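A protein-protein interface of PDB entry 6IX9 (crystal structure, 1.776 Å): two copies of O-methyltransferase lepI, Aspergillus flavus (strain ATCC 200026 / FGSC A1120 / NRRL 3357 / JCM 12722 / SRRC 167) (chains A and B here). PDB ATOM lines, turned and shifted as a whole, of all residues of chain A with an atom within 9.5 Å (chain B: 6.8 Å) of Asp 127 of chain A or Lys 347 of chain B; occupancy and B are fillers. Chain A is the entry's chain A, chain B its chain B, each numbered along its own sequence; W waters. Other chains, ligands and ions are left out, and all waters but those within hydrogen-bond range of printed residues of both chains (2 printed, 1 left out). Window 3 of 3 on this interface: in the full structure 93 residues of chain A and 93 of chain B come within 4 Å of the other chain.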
ATOM      1  N   PRO A  93      -5.130  13.564  -7.059  1.00  0.00           N
ATOM      2  CA  PRO A  93      -6.117  12.786  -7.825  1.00  0.00           C
ATOM      3  C   PRO A  93      -6.970  13.696  -8.694  1.00  0.00           C
ATOM      4  O   PRO A  93      -7.275  14.828  -8.318  1.00  0.00           O
ATOM      5  CB  PRO A  93      -6.955  12.100  -6.735  1.00  0.00           C
ATOM      6  CG  PRO A  93      -6.023  11.974  -5.559  1.00  0.00           C
ATOM      7  CD  PRO A  93      -5.194  13.276  -5.611  1.00  0.00           C
ATOM      8  N   ARG A 115     -13.143   3.966 -15.749  1.00  0.00           N
ATOM      9  CA  ARG A 115     -13.660   2.869 -14.940  1.00  0.00           C
ATOM     10  C   ARG A 115     -13.066   1.555 -15.397  1.00  0.00           C
ATOM     11  O   ARG A 115     -12.619   0.742 -14.581  1.00  0.00           O
ATOM     12  CB  ARG A 115     -15.187   2.805 -15.020  1.00  0.00           C
ATOM     13  CG  ARG A 115     -15.860   3.761 -14.075  1.00  0.00           C
ATOM     14  CD  ARG A 115     -17.363   3.876 -14.380  1.00  0.00           C
ATOM     15  NE  ARG A 115     -18.172   2.654 -14.217  1.00  0.00           N
ATOM     16  CZ  ARG A 115     -18.599   2.165 -13.050  1.00  0.00           C
ATOM     17  NH1 ARG A 115     -18.246   2.760 -11.920  1.00  0.00           N
ATOM     18  NH2 ARG A 115     -19.390   1.081 -13.009  1.00  0.00           N
ATOM     19  N   ALA A 118      -9.264   1.493 -14.558  1.00  0.00           N
ATOM     20  CA  ALA A 118      -8.980   1.245 -13.145  1.00  0.00           C
ATOM     21  C   ALA A 118      -9.170  -0.223 -12.804  1.00  0.00           C
ATOM     22  O   ALA A 118      -8.476  -0.755 -11.924  1.00  0.00           O
ATOM     23  CB  ALA A 118      -9.898   2.112 -12.264  1.00  0.00           C
ATOM     24  N   SER A 119     -10.102  -0.895 -13.480  1.00  0.00           N
ATOM     25  CA  SER A 119     -10.371  -2.301 -13.184  1.00  0.00           C
ATOM     26  C   SER A 119      -9.260  -3.225 -13.685  1.00  0.00           C
ATOM     27  O   SER A 119      -9.208  -4.393 -13.274  1.00  0.00           O
ATOM     28  CB  SER A 119     -11.726  -2.706 -13.786  1.00  0.00           C
ATOM     29  OG  SER A 119     -11.621  -2.912 -15.178  1.00  0.00           O
ATOM     30  N   GLN A 124      -5.332   4.023 -11.312  1.00  0.00           N
ATOM     31  CA  GLN A 124      -5.963   3.648 -10.048  1.00  0.00           C
ATOM     32  C   GLN A 124      -7.130   4.569  -9.743  1.00  0.00           C
ATOM     33  O   GLN A 124      -7.058   5.775  -9.979  1.00  0.00           O
ATOM     34  CB  GLN A 124      -4.986   3.668  -8.874  1.00  0.00           C
ATOM     35  CG  GLN A 124      -3.973   2.580  -8.970  1.00  0.00           C
ATOM     36  CD  GLN A 124      -3.308   2.337  -7.646  1.00  0.00           C
ATOM     37  OE1 GLN A 124      -3.524   1.305  -7.015  1.00  0.00           O
ATOM     38  NE2 GLN A 124      -2.511   3.300  -7.201  1.00  0.00           N
ATOM     39  N   GLN A 125      -8.219   3.986  -9.246  1.00  0.00           N
ATOM     40  CA  GLN A 125      -9.379   4.757  -8.828  1.00  0.00           C
ATOM     41  C   GLN A 125      -9.326   4.922  -7.315  1.00  0.00           C
ATOM     42  O   GLN A 125      -9.070   3.956  -6.598  1.00  0.00           O
ATOM     43  CB  GLN A 125     -10.667   4.052  -9.260  1.00  0.00           C
ATOM     44  CG  GLN A 125     -11.939   4.835  -9.030  1.00  0.00           C
ATOM     45  CD  GLN A 125     -13.132   3.915  -9.223  1.00  0.00           C
ATOM     46  OE1 GLN A 125     -13.331   2.996  -8.429  1.00  0.00           O
ATOM     47  NE2 GLN A 125     -13.902   4.126 -10.287  1.00  0.00           N
ATOM     48  N   THR A 126      -9.553   6.139  -6.830  1.00  0.00           N
ATOM     49  CA  THR A 126      -9.499   6.385  -5.397  1.00  0.00           C
ATOM     50  C   THR A 126     -10.869   6.177  -4.742  1.00  0.00           C
ATOM     51  O   THR A 126     -11.875   5.913  -5.401  1.00  0.00           O
ATOM     52  CB  THR A 126      -9.026   7.803  -5.094  1.00  0.00           C
ATOM     53  OG1 THR A 126     -10.042   8.719  -5.498  1.00  0.00           O
ATOM     54  CG2 THR A 126      -7.710   8.119  -5.815  1.00  0.00           C
ATOM     55  N   ASP A 127     -10.889   6.345  -3.417  1.00  0.00           N
ATOM     56  CA  ASP A 127     -12.148   6.088  -2.733  1.00  0.00           C
ATOM     57  C   ASP A 127     -13.202   7.159  -3.002  1.00  0.00           C
ATOM     58  O   ASP A 127     -14.409   6.859  -3.014  1.00  0.00           O
ATOM     59  CB  ASP A 127     -11.906   5.977  -1.230  1.00  0.00           C
ATOM     60  CG  ASP A 127     -12.983   5.202  -0.554  1.00  0.00           C
ATOM     61  OD1 ASP A 127     -13.325   4.109  -1.056  1.00  0.00           O
ATOM     62  OD2 ASP A 127     -13.503   5.691   0.471  1.00  0.00           O
ATOM     63  N   ASP A 128     -12.829   8.381  -3.372  1.00  0.00           N
ATOM     64  CA  ASP A 128     -13.806   9.373  -3.801  1.00  0.00           C
ATOM     65  C   ASP A 128     -13.934   9.413  -5.320  1.00  0.00           C
ATOM     66  O   ASP A 128     -14.274  10.455  -5.876  1.00  0.00           O
ATOM     67  CB  ASP A 128     -13.453  10.760  -3.246  1.00  0.00           C
ATOM     68  CG  ASP A 128     -12.035  11.155  -3.533  1.00  0.00           C
ATOM     69  OD1 ASP A 128     -11.365  10.458  -4.327  1.00  0.00           O
ATOM     70  OD2 ASP A 128     -11.556  12.144  -2.952  1.00  0.00           O
ATOM     71  N   ILE A 129     -13.680   8.287  -5.984  1.00  0.00           N
ATOM     72  CA  ILE A 129     -13.884   8.118  -7.419  1.00  0.00           C
ATOM     73  C   ILE A 129     -13.106   9.177  -8.194  1.00  0.00           C
ATOM     74  O   ILE A 129     -13.616   9.765  -9.157  1.00  0.00           O
ATOM     75  CB  ILE A 129     -15.379   8.142  -7.801  1.00  0.00           C
ATOM     76  CG1 ILE A 129     -16.226   7.428  -6.756  1.00  0.00           C
ATOM     77  CG2 ILE A 129     -15.615   7.388  -9.131  1.00  0.00           C
ATOM     78  CD1 ILE A 129     -17.717   7.369  -7.116  1.00  0.00           C
ATOM     79  N   LYS A 130     -11.862   9.408  -7.794  1.00  0.00           N
ATOM     80  CA  LYS A 130     -10.945  10.149  -8.636  1.00  0.00           C
ATOM     81  C   LYS A 130      -9.828   9.200  -9.060  1.00  0.00           C
ATOM     82  O   LYS A 130      -9.822   8.013  -8.683  1.00  0.00           O
ATOM     83  CB  LYS A 130     -10.418  11.381  -7.878  1.00  0.00           C
ATOM     84  CG  LYS A 130     -11.550  12.293  -7.359  1.00  0.00           C
ATOM     85  CD  LYS A 130     -11.023  13.399  -6.459  1.00  0.00           C
ATOM     86  CE  LYS A 130     -12.143  14.288  -5.921  1.00  0.00           C
ATOM     87  NZ  LYS A 130     -12.924  14.880  -7.030  1.00  0.00           N
ATOM     88  N   TYR A 131      -8.889   9.712  -9.858  1.00  0.00           N
ATOM     89  CA  TYR A 131      -7.951   8.842 -10.567  1.00  0.00           C
ATOM     90  C   TYR A 131      -6.511   9.331 -10.393  1.00  0.00           C
ATOM     91  O   TYR A 131      -6.241  10.540 -10.387  1.00  0.00           O
ATOM     92  CB  TYR A 131      -8.353   8.749 -12.059  1.00  0.00           C
ATOM     93  CG  TYR A 131      -9.721   8.091 -12.187  1.00  0.00           C
ATOM     94  CD1 TYR A 131      -9.834   6.709 -12.191  1.00  0.00           C
ATOM     95  CD2 TYR A 131     -10.896   8.847 -12.244  1.00  0.00           C
ATOM     96  CE1 TYR A 131     -11.084   6.081 -12.263  1.00  0.00           C
ATOM     97  CE2 TYR A 131     -12.151   8.220 -12.319  1.00  0.00           C
ATOM     98  CZ  TYR A 131     -12.236   6.836 -12.325  1.00  0.00           C
ATOM     99  OH  TYR A 131     -13.472   6.215 -12.392  1.00  0.00           O
ATOM    100  N   ILE A 132      -5.588   8.381 -10.217  1.00  0.00           N
ATOM    101  CA  ILE A 132      -4.164   8.646 -10.052  1.00  0.00           C
ATOM    102  C   ILE A 132      -3.435   7.647 -10.936  1.00  0.00           C
ATOM    103  O   ILE A 132      -3.990   6.625 -11.347  1.00  0.00           O
ATOM    104  CB  ILE A 132      -3.691   8.497  -8.583  1.00  0.00           C
ATOM    105  CG1 ILE A 132      -3.926   7.070  -8.079  1.00  0.00           C
ATOM    106  CG2 ILE A 132      -4.377   9.512  -7.652  1.00  0.00           C
ATOM    107  CD1 ILE A 132      -3.347   6.781  -6.684  1.00  0.00           C
ATOM    108  N   PRO B 344     -23.481  -2.959 -12.010  1.00  0.00           N
ATOM    109  CA  PRO B 344     -22.141  -2.676 -11.481  1.00  0.00           C
ATOM    110  C   PRO B 344     -22.183  -1.593 -10.440  1.00  0.00           C
ATOM    111  O   PRO B 344     -23.083  -0.727 -10.438  1.00  0.00           O
ATOM    112  CB  PRO B 344     -21.354  -2.230 -12.729  1.00  0.00           C
ATOM    113  CG  PRO B 344     -22.390  -1.851 -13.737  1.00  0.00           C
ATOM    114  CD  PRO B 344     -23.562  -2.756 -13.460  1.00  0.00           C
ATOM    115  N   PRO B 345     -21.223  -1.578  -9.515  1.00  0.00           N
ATOM    116  CA  PRO B 345     -21.209  -0.565  -8.455  1.00  0.00           C
ATOM    117  C   PRO B 345     -20.772   0.795  -8.978  1.00  0.00           C
ATOM    118  O   PRO B 345     -20.196   0.921 -10.065  1.00  0.00           O
ATOM    119  CB  PRO B 345     -20.193  -1.123  -7.452  1.00  0.00           C
ATOM    120  CG  PRO B 345     -19.213  -1.894  -8.332  1.00  0.00           C
ATOM    121  CD  PRO B 345     -20.118  -2.547  -9.388  1.00  0.00           C
ATOM    122  N   GLU B 346     -21.064   1.824  -8.171  1.00  0.00           N
ATOM    123  CA  GLU B 346     -20.618   3.183  -8.472  1.00  0.00           C
ATOM    124  C   GLU B 346     -19.102   3.307  -8.495  1.00  0.00           C
ATOM    125  O   GLU B 346     -18.562   4.121  -9.254  1.00  0.00           O
ATOM    126  CB  GLU B 346     -21.186   4.159  -7.436  1.00  0.00           C
ATOM    127  CG  GLU B 346     -22.703   4.111  -7.318  1.00  0.00           C
ATOM    128  CD  GLU B 346     -23.360   5.165  -8.182  1.00  0.00           C
ATOM    129  OE1 GLU B 346     -22.783   6.272  -8.300  1.00  0.00           O
ATOM    130  OE2 GLU B 346     -24.440   4.896  -8.740  1.00  0.00           O
ATOM    131  N   LYS B 347     -18.401   2.539  -7.656  1.00  0.00           N
ATOM    132  CA  LYS B 347     -16.947   2.544  -7.641  1.00  0.00           C
ATOM    133  C   LYS B 347     -16.437   1.127  -7.401  1.00  0.00           C
ATOM    134  O   LYS B 347     -17.143   0.256  -6.868  1.00  0.00           O
ATOM    135  CB  LYS B 347     -16.376   3.491  -6.578  1.00  0.00           C
ATOM    136  CG  LYS B 347     -16.523   2.984  -5.171  1.00  0.00           C
ATOM    137  CD  LYS B 347     -16.073   4.082  -4.186  1.00  0.00           C
ATOM    138  CE  LYS B 347     -16.409   3.741  -2.758  1.00  0.00           C
ATOM    139  NZ  LYS B 347     -16.022   4.877  -1.859  1.00  0.00           N
ATOM    140  N   GLY B 348     -15.185   0.915  -7.801  1.00  0.00           N
ATOM    141  CA  GLY B 348     -14.545  -0.380  -7.679  1.00  0.00           C
ATOM    142  C   GLY B 348     -15.123  -1.462  -8.572  1.00  0.00           C
ATOM    143  O   GLY B 348     -15.033  -2.650  -8.225  1.00  0.00           O
ATOM    144  N   ALA B 349     -15.704  -1.096  -9.718  1.00  0.00           N
ATOM    145  CA  ALA B 349     -16.266  -2.109 -10.603  1.00  0.00           C
ATOM    146  C   ALA B 349     -15.154  -2.994 -11.165  1.00  0.00           C
ATOM    147  O   ALA B 349     -14.032  -2.535 -11.407  1.00  0.00           O
ATOM    148  CB  ALA B 349     -17.076  -1.470 -11.747  1.00  0.00           C
ATOM    149  N   ARG B 350     -15.470  -4.267 -11.347  1.00  0.00           N
ATOM    150  CA  ARG B 350     -14.511  -5.299 -11.726  1.00  0.00           C
ATOM    151  C   ARG B 350     -14.349  -5.362 -13.242  1.00  0.00           C
ATOM    152  O   ARG B 350     -15.205  -4.884 -14.001  1.00  0.00           O
ATOM    153  CB  ARG B 350     -14.965  -6.671 -11.213  1.00  0.00           C
ATOM    154  CG  ARG B 350     -15.317  -6.784  -9.691  1.00  0.00           C
ATOM    155  CD  ARG B 350     -14.106  -6.581  -8.843  1.00  0.00           C
ATOM    156  NE  ARG B 350     -14.358  -6.662  -7.392  1.00  0.00           N
ATOM    157  CZ  ARG B 350     -13.853  -7.600  -6.583  1.00  0.00           C
ATOM    158  NH1 ARG B 350     -13.088  -8.575  -7.076  1.00  0.00           N
ATOM    159  NH2 ARG B 350     -14.087  -7.548  -5.271  1.00  0.00           N
ATOM    160  N   THR B 370     -25.510   1.205 -13.601  1.00  0.00           N
ATOM    161  CA  THR B 370     -25.585   1.113 -12.145  1.00  0.00           C
ATOM    162  C   THR B 370     -27.046   1.030 -11.699  1.00  0.00           C
ATOM    163  O   THR B 370     -27.977   1.232 -12.481  1.00  0.00           O
ATOM    164  CB  THR B 370     -24.952   2.335 -11.486  1.00  0.00           C
ATOM    165  OG1 THR B 370     -25.742   3.490 -11.823  1.00  0.00           O
ATOM    166  CG2 THR B 370     -23.472   2.505 -11.926  1.00  0.00           C
HETATM  167  O   HOH W   1     -13.577   0.347 -12.054  1.00  0.00           O
HETATM  168  O   HOH W   2     -17.651   5.561 -11.914  1.00  0.00           O
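Of chain B, only Lys 347 comes within 4 Å of Asp 127 of chain A. Lys 347 of chain B touches three residues of chain A. Pro 345 of chain B touches just one residue of chain A: Arg 115. Printed residues of chain A within 4 Å of Gly 348 of chain B: Gln 125 (2.9 Å). Of the printed residues of chain A, Arg 350 of chain B touches Ser 119 (3.8 Å). Printed residues of chain B within 4 Å of Ser 119 of chain A: Ala 349 and Arg 350. Of the printed residues of chain A, Glu 346 of chain B touches Arg 115 (3.0 Å) and Ile 129 (3.98 Å). Printed residues of chain A within 4 Å of Pro 344 of chain B: Arg 115. The nearest printed residue of chain B that does not touch Asp 127 of chain A is Gly 348 of chain B (7.7 Å). The nearest residue of chain A that does not touch Lys 347 of chain B is Arg 115 of chain A (4.3 Å).
Water W1 bridges the backbone carbonyl oxygen of Arg 115 of chain A (2.7 Å) and the backbone carbonyl oxygen of Ala 349 of chain B (3.0 Å). Water W2 lies within hydrogen-bond range of the guanidinium group (NH1) of Arg 115 of chain A (2.9 Å) and the backbone carbonyl oxygen (O) of Glu 346 of chain B (3.2 Å).
The side-chain amide nitrogen of Gln 125 of chain A is in hydrogen-bond range of the side-chain hydroxyl of Tyr 131 of chain A (3.0 Å).
No position is printed for both chains. Of the 11 pairs that touch across the chains among the printed residues, none has its exchanged pair printed and touching as well.
The guanidinium group (NH2) of Arg 115 of chain A sits at hydrogen-bond distance from the backbone carbonyl oxygen (O) of Pro 345 of chain B, at 3.1 Å. The side-chain carboxylate (OD1) of Asp 127 of chain A is in salt-bridge range of the side-chain amino group (NZ) of Lys 347 of chain B (2.9 Å). N of Gly 348 of chain B sits at hydrogen-bond distance from OE1 of Gln 125 of chain A (2.9 Å). The backbone carbonyl oxygen (O) of Glu 346 of chain B is in hydrogen-bond range of the guanidinium group (NH1) of Arg 115 of chain A (3.0 Å).
Of the 8 printed residues of chain B, 7 touch a printed residue of chain A. Hydrophobic or aromatic side chains of chain A that line the printed part of chain B: Ile 129. Among the printed residues, 11 pairs touch across the chains. Among the printed residues, Asp or Glu carboxylates within 4 Å of a Lys or Arg side-chain nitrogen of the other chain: Asp 127 of chain A with Lys 347 of chain B (2.9 Å).
Arg 115 of chain A touches Pro 344 of chain B (NH2 to CB, 3.9 Å). CB of Ala 349 of chain B touches NH2 of Arg 115 of chain A, 3.7 Å away. CB of Ser 119 of chain A touches O of Ala 349 of chain B, 3.3 Å away. Arg 350 of chain B touches Ser 119 of chain A (C to CB, 3.8 Å). Lys 347 of chain B touches Gln 125 of chain A. O of Glu 346 of chain B touches CD1 of Ile 129 of chain A (3.98 Å). Lys 347 of chain B touches Ile 129 of chain A.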
